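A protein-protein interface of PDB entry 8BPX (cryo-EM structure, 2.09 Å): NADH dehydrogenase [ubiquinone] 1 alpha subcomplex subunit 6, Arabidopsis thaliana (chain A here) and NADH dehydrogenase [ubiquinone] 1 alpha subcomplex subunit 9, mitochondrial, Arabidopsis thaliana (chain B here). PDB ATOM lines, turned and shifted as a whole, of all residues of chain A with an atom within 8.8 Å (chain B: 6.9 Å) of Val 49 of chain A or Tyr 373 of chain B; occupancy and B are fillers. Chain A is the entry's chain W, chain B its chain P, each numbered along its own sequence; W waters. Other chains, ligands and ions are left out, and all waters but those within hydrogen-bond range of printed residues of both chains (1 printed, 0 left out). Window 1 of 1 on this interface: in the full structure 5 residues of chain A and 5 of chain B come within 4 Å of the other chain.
N of Leu 46 of chain A lies within hydrogen-bond range of O of Met 41 of chain A (3.1 Å). O of His 98 of chain A is in hydrogen-bond range of N of Val 105 of chain A, 2.5 Å away.
O of His 97 of chain A sits at hydrogen-bond distance from OH of Tyr 373 of chain B (2.4 Å). OE1 of Glu 376 of chain B is in hydrogen-bond range of NE2 of His 97 of chain A (3.3 Å).
Water W1 bridges NE2 of His 98 of chain A (2.7 Å) and NE2 of His 368 of chain B (3.3 Å).
Val 49 of chain A touches one residue of chain B. Gly 372 of chain B touches one residue of chain A. No residue of chain A comes within 4 Å of Pro 374 of chain B. Of the printed residues of chain B, His 97 of chain A touches Tyr 257, Tyr 373 and Glu 376. Of the printed residues of chain B, His 98 of chain A touches His 368 (3.7 Å). Printed residues of chain A within 4 Å of Glu 376 of chain B: His 97. Of the printed residues of chain B, Leu 46 of chain A touches Tyr 373. Of the printed residues of chain A, His 368 of chain B touches His 98. The nearest residue of chain B that does not touch Val 49 of chain A is Gly 372 of chain B (4.8 Å). The nearest printed residue of chain B that does not touch His 98 of chain A is Tyr 373 of chain B (4.1 Å).
CD2 of Leu 46 of chain A touches OH of Tyr 373 of chain B, at 3.4 Å. N of Gly 372 of chain B touches OD2 of Asp 48 of chain A (3.9 Å). CZ of Tyr 373 of chain B touches CG2 of Val 49 of chain A, 3.9 Å away. CE1 of His 97 of chain A touches OH of Tyr 257 of chain B, at 3.98 Å. His 98 of chain A touches His 368 of chain B (NE2 to NE2, 3.7 Å).
Of the 12 printed residues of chain B, 5 touch a printed residue of chain A. Along chain B the printed residues that touch a printed residue of chain A span positions 257 to 376.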
ATOM      1  N   ILE A  40     -24.192 -19.667 -20.946  1.00  0.00           N
ATOM      2  CA  ILE A  40     -22.824 -19.298 -21.295  1.00  0.00           C
ATOM      3  C   ILE A  40     -22.501 -17.891 -20.807  1.00  0.00           C
ATOM      4  O   ILE A  40     -21.405 -17.636 -20.292  1.00  0.00           O
ATOM      5  CB  ILE A  40     -22.618 -19.441 -22.812  1.00  0.00           C
ATOM      6  CG1 ILE A  40     -22.558 -20.924 -23.188  1.00  0.00           C
ATOM      7  CG2 ILE A  40     -21.363 -18.707 -23.258  1.00  0.00           C
ATOM      8  CD1 ILE A  40     -22.823 -21.203 -24.637  1.00  0.00           C
ATOM      9  N   MET A  41     -23.441 -16.956 -20.962  1.00  0.00           N
ATOM     10  CA  MET A  41     -23.217 -15.597 -20.482  1.00  0.00           C
ATOM     11  C   MET A  41     -22.977 -15.585 -18.982  1.00  0.00           C
ATOM     12  O   MET A  41     -22.089 -14.876 -18.493  1.00  0.00           O
ATOM     13  CB  MET A  41     -24.406 -14.700 -20.832  1.00  0.00           C
ATOM     14  CG  MET A  41     -24.690 -14.558 -22.314  1.00  0.00           C
ATOM     15  SD  MET A  41     -23.739 -13.245 -23.093  1.00  0.00           S
ATOM     16  CE  MET A  41     -24.429 -11.798 -22.293  1.00  0.00           C
ATOM     17  N   ILE A  43     -21.875 -18.203 -17.120  1.00  0.00           N
ATOM     18  CA  ILE A  43     -20.684 -18.967 -16.755  1.00  0.00           C
ATOM     19  C   ILE A  43     -19.421 -18.151 -17.005  1.00  0.00           C
ATOM     20  O   ILE A  43     -18.499 -18.137 -16.181  1.00  0.00           O
ATOM     21  CB  ILE A  43     -20.655 -20.308 -17.515  1.00  0.00           C
ATOM     22  CG1 ILE A  43     -21.464 -21.363 -16.765  1.00  0.00           C
ATOM     23  CG2 ILE A  43     -19.232 -20.796 -17.693  1.00  0.00           C
ATOM     24  CD1 ILE A  43     -21.665 -22.646 -17.540  1.00  0.00           C
ATOM     25  N   TYR A  44     -19.359 -17.454 -18.135  1.00  0.00           N
ATOM     26  CA  TYR A  44     -18.182 -16.681 -18.507  1.00  0.00           C
ATOM     27  C   TYR A  44     -18.255 -15.218 -18.074  1.00  0.00           C
ATOM     28  O   TYR A  44     -17.326 -14.462 -18.371  1.00  0.00           O
ATOM     29  CB  TYR A  44     -17.953 -16.759 -20.022  1.00  0.00           C
ATOM     30  CG  TYR A  44     -17.683 -18.154 -20.555  1.00  0.00           C
ATOM     31  CD1 TYR A  44     -18.707 -19.080 -20.698  1.00  0.00           C
ATOM     32  CD2 TYR A  44     -16.403 -18.539 -20.930  1.00  0.00           C
ATOM     33  CE1 TYR A  44     -18.464 -20.347 -21.182  1.00  0.00           C
ATOM     34  CE2 TYR A  44     -16.151 -19.805 -21.419  1.00  0.00           C
ATOM     35  CZ  TYR A  44     -17.182 -20.705 -21.543  1.00  0.00           C
ATOM     36  OH  TYR A  44     -16.938 -21.966 -22.030  1.00  0.00           O
ATOM     37  N   ASN A  45     -19.323 -14.802 -17.392  1.00  0.00           N
ATOM     38  CA  ASN A  45     -19.486 -13.421 -16.923  1.00  0.00           C
ATOM     39  C   ASN A  45     -19.338 -12.426 -18.072  1.00  0.00           C
ATOM     40  O   ASN A  45     -18.433 -11.594 -18.104  1.00  0.00           O
ATOM     41  CB  ASN A  45     -18.500 -13.100 -15.797  1.00  0.00           C
ATOM     42  CG  ASN A  45     -18.424 -14.196 -14.766  1.00  0.00           C
ATOM     43  OD1 ASN A  45     -19.293 -14.313 -13.907  1.00  0.00           O
ATOM     44  ND2 ASN A  45     -17.380 -15.013 -14.845  1.00  0.00           N
ATOM     45  N   LEU A  46     -20.267 -12.481 -19.003  1.00  0.00           N
ATOM     46  CA  LEU A  46     -20.044 -11.665 -20.207  1.00  0.00           C
ATOM     47  C   LEU A  46     -20.946 -10.457 -20.265  1.00  0.00           C
ATOM     48  O   LEU A  46     -20.804  -9.745 -21.218  1.00  0.00           O
ATOM     49  CB  LEU A  46     -20.200 -12.596 -21.418  1.00  0.00           C
ATOM     50  CG  LEU A  46     -19.105 -13.640 -21.595  1.00  0.00           C
ATOM     51  CD1 LEU A  46     -19.460 -14.616 -22.698  1.00  0.00           C
ATOM     52  CD2 LEU A  46     -17.769 -12.994 -21.867  1.00  0.00           C
ATOM     53  N   GLN A  47     -21.730 -10.210 -19.198  1.00  0.00           N
ATOM     54  CA  GLN A  47     -22.747  -9.162 -19.234  1.00  0.00           C
ATOM     55  C   GLN A  47     -22.171  -7.842 -19.729  1.00  0.00           C
ATOM     56  O   GLN A  47     -22.795  -7.152 -20.544  1.00  0.00           O
ATOM     57  CB  GLN A  47     -23.394  -8.976 -17.856  1.00  0.00           C
ATOM     58  CG  GLN A  47     -24.068 -10.204 -17.204  1.00  0.00           C
ATOM     59  CD  GLN A  47     -23.159 -11.395 -16.941  1.00  0.00           C
ATOM     60  OE1 GLN A  47     -22.013 -11.439 -17.378  1.00  0.00           O
ATOM     61  NE2 GLN A  47     -23.680 -12.375 -16.209  1.00  0.00           N
ATOM     62  N   ASP A  48     -20.979  -7.479 -19.267  1.00  0.00           N
ATOM     63  CA  ASP A  48     -20.358  -6.220 -19.648  1.00  0.00           C
ATOM     64  C   ASP A  48     -19.302  -6.400 -20.730  1.00  0.00           C
ATOM     65  O   ASP A  48     -18.450  -5.523 -20.902  1.00  0.00           O
ATOM     66  CB  ASP A  48     -19.752  -5.544 -18.419  1.00  0.00           C
ATOM     67  CG  ASP A  48     -20.727  -5.470 -17.261  1.00  0.00           C
ATOM     68  OD1 ASP A  48     -21.948  -5.578 -17.505  1.00  0.00           O
ATOM     69  OD2 ASP A  48     -20.274  -5.307 -16.109  1.00  0.00           O
ATOM     70  N   VAL A  49     -19.369  -7.513 -21.481  1.00  0.00           N
ATOM     71  CA  VAL A  49     -18.312  -7.814 -22.498  1.00  0.00           C
ATOM     72  C   VAL A  49     -18.879  -7.927 -23.915  1.00  0.00           C
ATOM     73  O   VAL A  49     -18.186  -7.510 -24.813  1.00  0.00           O
ATOM     74  CB  VAL A  49     -17.589  -9.118 -22.138  1.00  0.00           C
ATOM     75  CG1 VAL A  49     -16.600  -9.555 -23.207  1.00  0.00           C
ATOM     76  CG2 VAL A  49     -16.898  -9.042 -20.789  1.00  0.00           C
ATOM     77  N   VAL A  50     -20.081  -8.465 -24.058  1.00  0.00           N
ATOM     78  CA  VAL A  50     -20.655  -8.756 -25.399  1.00  0.00           C
ATOM     79  C   VAL A  50     -22.136  -9.060 -25.246  1.00  0.00           C
ATOM     80  O   VAL A  50     -22.532  -9.552 -24.219  1.00  0.00           O
ATOM     81  CB  VAL A  50     -19.946  -9.973 -26.032  1.00  0.00           C
ATOM     82  CG1 VAL A  50     -20.419 -11.287 -25.440  1.00  0.00           C
ATOM     83  CG2 VAL A  50     -20.076  -9.996 -27.545  1.00  0.00           C
ATOM     84  N   ALA A  51     -22.929  -8.719 -26.256  1.00  0.00           N
ATOM     85  CA  ALA A  51     -24.363  -8.953 -26.269  1.00  0.00           C
ATOM     86  C   ALA A  51     -24.676 -10.400 -26.644  1.00  0.00           C
ATOM     87  O   ALA A  51     -23.925 -11.027 -27.397  1.00  0.00           O
ATOM     88  CB  ALA A  51     -25.045  -8.016 -27.260  1.00  0.00           C
ATOM     89  N   PRO A  52     -25.780 -10.951 -26.127  1.00  0.00           N
ATOM     90  CA  PRO A  52     -26.163 -12.320 -26.515  1.00  0.00           C
ATOM     91  C   PRO A  52     -26.396 -12.487 -28.005  1.00  0.00           C
ATOM     92  O   PRO A  52     -26.118 -13.563 -28.550  1.00  0.00           O
ATOM     93  CB  PRO A  52     -27.449 -12.560 -25.710  1.00  0.00           C
ATOM     94  CG  PRO A  52     -27.338 -11.644 -24.550  1.00  0.00           C
ATOM     95  CD  PRO A  52     -26.631 -10.423 -25.049  1.00  0.00           C
ATOM     96  N   GLN A  54     -24.761 -11.218 -30.447  1.00  0.00           N
ATOM     97  CA  GLN A  54     -23.491 -11.465 -31.116  1.00  0.00           C
ATOM     98  C   GLN A  54     -23.104 -12.938 -31.046  1.00  0.00           C
ATOM     99  O   GLN A  54     -22.518 -13.468 -31.993  1.00  0.00           O
ATOM    100  CB  GLN A  54     -22.403 -10.583 -30.502  1.00  0.00           C
ATOM    101  CG  GLN A  54     -22.675  -9.098 -30.662  1.00  0.00           C
ATOM    102  CD  GLN A  54     -21.412  -8.289 -30.875  1.00  0.00           C
ATOM    103  OE1 GLN A  54     -20.858  -7.725 -29.933  1.00  0.00           O
ATOM    104  NE2 GLN A  54     -20.950  -8.229 -32.118  1.00  0.00           N
ATOM    105  N   LEU A  55     -23.366 -13.574 -29.929  1.00  0.00           N
ATOM    106  CA  LEU A  55     -23.192 -15.051 -29.842  1.00  0.00           C
ATOM    107  C   LEU A  55     -24.099 -15.748 -30.865  1.00  0.00           C
ATOM    108  O   LEU A  55     -23.597 -16.559 -31.589  1.00  0.00           O
ATOM    109  CB  LEU A  55     -23.600 -15.473 -28.440  1.00  0.00           C
ATOM    110  CG  LEU A  55     -22.581 -15.079 -27.370  1.00  0.00           C
ATOM    111  CD1 LEU A  55     -22.720 -15.939 -26.135  1.00  0.00           C
ATOM    112  CD2 LEU A  55     -21.180 -15.199 -27.927  1.00  0.00           C
ATOM    113  N   GLN A  95     -12.500 -20.864 -19.074  1.00  0.00           N
ATOM    114  CA  GLN A  95     -12.499 -19.385 -19.182  1.00  0.00           C
ATOM    115  C   GLN A  95     -11.168 -18.772 -19.622  1.00  0.00           C
ATOM    116  O   GLN A  95     -10.169 -19.100 -19.031  1.00  0.00           O
ATOM    117  CB  GLN A  95     -12.824 -18.853 -17.811  1.00  0.00           C
ATOM    118  CG  GLN A  95     -14.302 -18.992 -17.445  1.00  0.00           C
ATOM    119  CD  GLN A  95     -14.520 -19.887 -16.250  1.00  0.00           C
ATOM    120  OE1 GLN A  95     -13.612 -20.582 -15.796  1.00  0.00           O
ATOM    121  NE2 GLN A  95     -15.732 -19.878 -15.723  1.00  0.00           N
ATOM    122  N   ARG A  96     -11.145 -17.967 -20.673  1.00  0.00           N
ATOM    123  CA  ARG A  96      -9.989 -17.115 -21.014  1.00  0.00           C
ATOM    124  C   ARG A  96     -10.606 -15.719 -20.844  1.00  0.00           C
ATOM    125  O   ARG A  96     -11.375 -15.545 -19.911  1.00  0.00           O
ATOM    126  CB  ARG A  96      -9.327 -17.419 -22.366  1.00  0.00           C
ATOM    127  CG  ARG A  96      -8.746 -18.811 -22.463  1.00  0.00           C
ATOM    128  CD  ARG A  96      -7.634 -18.901 -21.445  1.00  0.00           C
ATOM    129  NE  ARG A  96      -6.507 -17.990 -21.587  1.00  0.00           N
ATOM    130  CZ  ARG A  96      -5.468 -18.164 -22.399  1.00  0.00           C
ATOM    131  NH1 ARG A  96      -5.388 -19.218 -23.192  1.00  0.00           N
ATOM    132  NH2 ARG A  96      -4.496 -17.272 -22.409  1.00  0.00           N
ATOM    133  N   HIS A  97     -10.167 -14.741 -21.616  1.00  0.00           N
ATOM    134  CA  HIS A  97     -10.842 -13.437 -21.446  1.00  0.00           C
ATOM    135  C   HIS A  97     -11.695 -13.200 -22.680  1.00  0.00           C
ATOM    136  O   HIS A  97     -12.901 -13.475 -22.638  1.00  0.00           O
ATOM    137  CB  HIS A  97      -9.815 -12.323 -21.203  1.00  0.00           C
ATOM    138  CG  HIS A  97      -9.629 -11.993 -19.761  1.00  0.00           C
ATOM    139  ND1 HIS A  97      -9.311 -10.719 -19.330  1.00  0.00           N
ATOM    140  CD2 HIS A  97      -9.728 -12.755 -18.651  1.00  0.00           C
ATOM    141  CE1 HIS A  97      -9.214 -10.715 -18.016  1.00  0.00           C
ATOM    142  NE2 HIS A  97      -9.465 -11.952 -17.575  1.00  0.00           N
ATOM    143  N   HIS A  98     -11.051 -12.848 -23.779  1.00  0.00           N
ATOM    144  CA  HIS A  98     -11.811 -12.455 -24.971  1.00  0.00           C
ATOM    145  C   HIS A  98     -12.085 -13.653 -25.849  1.00  0.00           C
ATOM    146  O   HIS A  98     -12.396 -13.464 -27.001  1.00  0.00           O
ATOM    147  CB  HIS A  98     -10.849 -11.563 -25.653  1.00  0.00           C
ATOM    148  CG  HIS A  98     -10.942 -10.209 -25.040  1.00  0.00           C
ATOM    149  ND1 HIS A  98     -12.070  -9.449 -25.173  1.00  0.00           N
ATOM    150  CD2 HIS A  98     -10.104  -9.516 -24.245  1.00  0.00           C
ATOM    151  CE1 HIS A  98     -11.916  -8.318 -24.535  1.00  0.00           C
ATOM    152  NE2 HIS A  98     -10.721  -8.330 -23.960  1.00  0.00           N
ATOM    153  N   ILE A  99     -12.019 -14.836 -25.287  1.00  0.00           N
ATOM    154  CA  ILE A  99     -12.083 -16.053 -26.144  1.00  0.00           C
ATOM    155  C   ILE A  99     -12.991 -17.102 -25.512  1.00  0.00           C
ATOM    156  O   ILE A  99     -12.721 -17.446 -24.375  1.00  0.00           O
ATOM    157  CB  ILE A  99     -10.654 -16.620 -26.302  1.00  0.00           C
ATOM    158  CG1 ILE A  99      -9.770 -15.759 -27.205  1.00  0.00           C
ATOM    159  CG2 ILE A  99     -10.690 -18.062 -26.784  1.00  0.00           C
ATOM    160  CD1 ILE A  99      -8.295 -16.049 -27.063  1.00  0.00           C
ATOM    161  N   ILE A 100     -13.998 -17.597 -26.223  1.00  0.00           N
ATOM    162  CA  ILE A 100     -14.791 -18.776 -25.739  1.00  0.00           C
ATOM    163  C   ILE A 100     -14.498 -19.919 -26.721  1.00  0.00           C
ATOM    164  O   ILE A 100     -14.677 -19.689 -27.898  1.00  0.00           O
ATOM    165  CB  ILE A 100     -16.307 -18.538 -25.709  1.00  0.00           C
ATOM    166  CG1 ILE A 100     -16.710 -17.372 -24.807  1.00  0.00           C
ATOM    167  CG2 ILE A 100     -17.019 -19.807 -25.288  1.00  0.00           C
ATOM    168  CD1 ILE A 100     -18.100 -16.877 -25.093  1.00  0.00           C
ATOM    169  N   VAL A 104     -13.323 -15.662 -30.803  1.00  0.00           N
ATOM    170  CA  VAL A 104     -12.875 -14.452 -30.111  1.00  0.00           C
ATOM    171  C   VAL A 104     -14.168 -13.731 -29.725  1.00  0.00           C
ATOM    172  O   VAL A 104     -14.907 -13.395 -30.616  1.00  0.00           O
ATOM    173  CB  VAL A 104     -12.074 -13.523 -31.031  1.00  0.00           C
ATOM    174  CG1 VAL A 104     -11.341 -12.458 -30.231  1.00  0.00           C
ATOM    175  CG2 VAL A 104     -11.090 -14.300 -31.897  1.00  0.00           C
ATOM    176  N   VAL A 105     -14.419 -13.581 -28.440  1.00  0.00           N
ATOM    177  CA  VAL A 105     -15.689 -12.939 -27.957  1.00  0.00           C
ATOM    178  C   VAL A 105     -15.332 -11.545 -27.468  1.00  0.00           C
ATOM    179  O   VAL A 105     -14.159 -11.231 -27.353  1.00  0.00           O
ATOM    180  CB  VAL A 105     -16.407 -13.664 -26.807  1.00  0.00           C
ATOM    181  CG1 VAL A 105     -15.869 -13.344 -25.421  1.00  0.00           C
ATOM    182  CG2 VAL A 105     -17.920 -13.528 -26.868  1.00  0.00           C
ATOM    183  N   GLY A 106     -16.348 -10.773 -27.096  1.00  0.00           N
ATOM    184  CA  GLY A 106     -16.037  -9.374 -26.779  1.00  0.00           C
ATOM    185  C   GLY A 106     -15.273  -8.757 -27.930  1.00  0.00           C
ATOM    186  O   GLY A 106     -14.930  -7.570 -27.806  1.00  0.00           O
ATOM    187  N   TYR B 257      -6.684   0.169 -15.884  1.00  0.00           N
ATOM    188  CA  TYR B 257      -6.310  -1.239 -15.815  1.00  0.00           C
ATOM    189  C   TYR B 257      -4.794  -1.385 -15.744  1.00  0.00           C
ATOM    190  O   TYR B 257      -4.063  -0.789 -16.539  1.00  0.00           O
ATOM    191  CB  TYR B 257      -6.859  -1.970 -17.039  1.00  0.00           C
ATOM    192  CG  TYR B 257      -6.917  -3.476 -16.929  1.00  0.00           C
ATOM    193  CD1 TYR B 257      -6.981  -4.114 -15.697  1.00  0.00           C
ATOM    194  CD2 TYR B 257      -6.895  -4.263 -18.071  1.00  0.00           C
ATOM    195  CE1 TYR B 257      -7.031  -5.499 -15.612  1.00  0.00           C
ATOM    196  CE2 TYR B 257      -6.946  -5.637 -17.998  1.00  0.00           C
ATOM    197  CZ  TYR B 257      -7.014  -6.253 -16.772  1.00  0.00           C
ATOM    198  OH  TYR B 257      -7.063  -7.627 -16.715  1.00  0.00           O
ATOM    199  N   MET B 300     -20.679  -5.444  -8.939  1.00  0.00           N
ATOM    200  CA  MET B 300     -19.841  -6.657  -8.969  1.00  0.00           C
ATOM    201  C   MET B 300     -19.880  -7.470  -7.676  1.00  0.00           C
ATOM    202  O   MET B 300     -19.839  -8.673  -7.783  1.00  0.00           O
ATOM    203  CB  MET B 300     -18.368  -6.287  -9.230  1.00  0.00           C
ATOM    204  CG  MET B 300     -18.096  -5.739 -10.594  1.00  0.00           C
ATOM    205  SD  MET B 300     -18.514  -6.915 -11.880  1.00  0.00           S
ATOM    206  CE  MET B 300     -17.367  -8.241 -11.501  1.00  0.00           C
ATOM    207  N   HIS B 368      -8.208  -0.240 -21.710  1.00  0.00           N
ATOM    208  CA  HIS B 368      -9.387  -1.065 -21.504  1.00  0.00           C
ATOM    209  C   HIS B 368     -10.341  -0.399 -20.516  1.00  0.00           C
ATOM    210  O   HIS B 368      -9.921   0.259 -19.561  1.00  0.00           O
ATOM    211  CB  HIS B 368      -8.977  -2.450 -20.997  1.00  0.00           C
ATOM    212  CG  HIS B 368      -9.993  -3.524 -21.248  1.00  0.00           C
ATOM    213  ND1 HIS B 368     -11.329  -3.375 -20.948  1.00  0.00           N
ATOM    214  CD2 HIS B 368      -9.863  -4.761 -21.780  1.00  0.00           C
ATOM    215  CE1 HIS B 368     -11.979  -4.477 -21.279  1.00  0.00           C
ATOM    216  NE2 HIS B 368     -11.112  -5.334 -21.785  1.00  0.00           N
ATOM    217  N   LYS B 369     -11.636  -0.562 -20.766  1.00  0.00           N
ATOM    218  CA  LYS B 369     -12.653  -0.066 -19.851  1.00  0.00           C
ATOM    219  C   LYS B 369     -12.739  -0.953 -18.614  1.00  0.00           C
ATOM    220  O   LYS B 369     -12.519  -2.165 -18.675  1.00  0.00           O
ATOM    221  CB  LYS B 369     -14.009   0.008 -20.550  1.00  0.00           C
ATOM    222  CG  LYS B 369     -14.435   1.423 -20.897  1.00  0.00           C
ATOM    223  CD  LYS B 369     -15.513   1.438 -21.968  1.00  0.00           C
ATOM    224  CE  LYS B 369     -15.590   2.797 -22.645  1.00  0.00           C
ATOM    225  NZ  LYS B 369     -14.752   2.855 -23.874  1.00  0.00           N
ATOM    226  N   LEU B 370     -13.059  -0.329 -17.477  1.00  0.00           N
ATOM    227  CA  LEU B 370     -12.960  -1.016 -16.192  1.00  0.00           C
ATOM    228  C   LEU B 370     -13.998  -2.126 -16.058  1.00  0.00           C
ATOM    229  O   LEU B 370     -13.686  -3.228 -15.592  1.00  0.00           O
ATOM    230  CB  LEU B 370     -13.100  -0.013 -15.047  1.00  0.00           C
ATOM    231  CG  LEU B 370     -11.926   0.940 -14.812  1.00  0.00           C
ATOM    232  CD1 LEU B 370     -11.852   1.331 -13.348  1.00  0.00           C
ATOM    233  CD2 LEU B 370     -10.619   0.315 -15.268  1.00  0.00           C
ATOM    234  N   LYS B 371     -15.243  -1.848 -16.442  1.00  0.00           N
ATOM    235  CA  LYS B 371     -16.333  -2.790 -16.209  1.00  0.00           C
ATOM    236  C   LYS B 371     -16.072  -4.126 -16.889  1.00  0.00           C
ATOM    237  O   LYS B 371     -15.607  -4.180 -18.028  1.00  0.00           O
ATOM    238  CB  LYS B 371     -17.653  -2.205 -16.705  1.00  0.00           C
ATOM    239  CG  LYS B 371     -18.439  -1.468 -15.645  1.00  0.00           C
ATOM    240  CD  LYS B 371     -19.336  -0.409 -16.266  1.00  0.00           C
ATOM    241  CE  LYS B 371     -20.621  -0.240 -15.473  1.00  0.00           C
ATOM    242  NZ  LYS B 371     -21.554   0.725 -16.117  1.00  0.00           N
ATOM    243  N   GLY B 372     -16.361  -5.200 -16.170  1.00  0.00           N
ATOM    244  CA  GLY B 372     -16.196  -6.542 -16.700  1.00  0.00           C
ATOM    245  C   GLY B 372     -14.857  -7.144 -16.301  1.00  0.00           C
ATOM    246  O   GLY B 372     -14.638  -7.476 -15.137  1.00  0.00           O
ATOM    247  N   TYR B 373     -13.965  -7.285 -17.279  1.00  0.00           N
ATOM    248  CA  TYR B 373     -12.731  -8.041 -17.067  1.00  0.00           C
ATOM    249  C   TYR B 373     -11.787  -7.397 -16.059  1.00  0.00           C
ATOM    250  O   TYR B 373     -11.279  -8.118 -15.183  1.00  0.00           O
ATOM    251  CB  TYR B 373     -12.072  -8.272 -18.427  1.00  0.00           C
ATOM    252  CG  TYR B 373     -12.685  -9.444 -19.127  1.00  0.00           C
ATOM    253  CD1 TYR B 373     -13.430 -10.373 -18.418  1.00  0.00           C
ATOM    254  CD2 TYR B 373     -12.626  -9.563 -20.500  1.00  0.00           C
ATOM    255  CE1 TYR B 373     -14.024 -11.433 -19.042  1.00  0.00           C
ATOM    256  CE2 TYR B 373     -13.229 -10.611 -21.137  1.00  0.00           C
ATOM    257  CZ  TYR B 373     -13.927 -11.550 -20.403  1.00  0.00           C
ATOM    258  OH  TYR B 373     -14.533 -12.612 -21.032  1.00  0.00           O
ATOM    259  N   PRO B 374     -11.498  -6.090 -16.111  1.00  0.00           N
ATOM    260  CA  PRO B 374     -10.625  -5.509 -15.077  1.00  0.00           C
ATOM    261  C   PRO B 374     -11.156  -5.654 -13.660  1.00  0.00           C
ATOM    262  O   PRO B 374     -10.355  -5.725 -12.720  1.00  0.00           O
ATOM    263  CB  PRO B 374     -10.525  -4.039 -15.501  1.00  0.00           C
ATOM    264  CG  PRO B 374     -10.660  -4.094 -16.969  1.00  0.00           C
ATOM    265  CD  PRO B 374     -11.719  -5.133 -17.210  1.00  0.00           C
ATOM    266  N   VAL B 375     -12.475  -5.699 -13.468  1.00  0.00           N
ATOM    267  CA  VAL B 375     -13.057  -5.874 -12.142  1.00  0.00           C
ATOM    268  C   VAL B 375     -13.520  -7.308 -11.908  1.00  0.00           C
ATOM    269  O   VAL B 375     -14.210  -7.579 -10.921  1.00  0.00           O
ATOM    270  CB  VAL B 375     -14.211  -4.885 -11.907  1.00  0.00           C
ATOM    271  CG1 VAL B 375     -13.693  -3.453 -11.873  1.00  0.00           C
ATOM    272  CG2 VAL B 375     -15.270  -5.044 -12.982  1.00  0.00           C
ATOM    273  N   GLU B 376     -13.359  -8.244 -12.822  1.00  0.00           N
ATOM    274  CA  GLU B 376     -13.730  -9.672 -12.591  1.00  0.00           C
ATOM    275  C   GLU B 376     -13.116 -10.271 -11.306  1.00  0.00           C
ATOM    276  O   GLU B 376     -13.730 -11.152 -10.731  1.00  0.00           O
ATOM    277  CB  GLU B 376     -13.196 -10.492 -13.735  1.00  0.00           C
ATOM    278  CG  GLU B 376     -13.693 -11.921 -13.790  1.00  0.00           C
ATOM    279  CD  GLU B 376     -12.943 -12.765 -14.804  1.00  0.00           C
ATOM    280  OE1 GLU B 376     -11.934 -12.273 -15.347  1.00  0.00           O
ATOM    281  OE2 GLU B 376     -13.369 -13.912 -15.046  1.00  0.00           O
ATOM    282  N   PHE B 377     -11.983  -9.796 -10.832  1.00  0.00           N
ATOM    283  CA  PHE B 377     -11.495 -10.356  -9.578  1.00  0.00           C
ATOM    284  C   PHE B 377     -12.463 -10.124  -8.425  1.00  0.00           C
ATOM    285  O   PHE B 377     -12.378 -10.825  -7.411  1.00  0.00           O
ATOM    286  CB  PHE B 377     -10.125  -9.774  -9.235  1.00  0.00           C
ATOM    287  CG  PHE B 377     -10.166  -8.332  -8.824  1.00  0.00           C
ATOM    288  CD1 PHE B 377     -10.232  -7.331  -9.776  1.00  0.00           C
ATOM    289  CD2 PHE B 377     -10.137  -7.977  -7.486  1.00  0.00           C
ATOM    290  CE1 PHE B 377     -10.270  -6.003  -9.402  1.00  0.00           C
ATOM    291  CE2 PHE B 377     -10.176  -6.654  -7.108  1.00  0.00           C
ATOM    292  CZ  PHE B 377     -10.243  -5.667  -8.068  1.00  0.00           C
HETATM  293  O   HOH W   1      -8.749  -7.565 -22.257  1.00  0.00           O
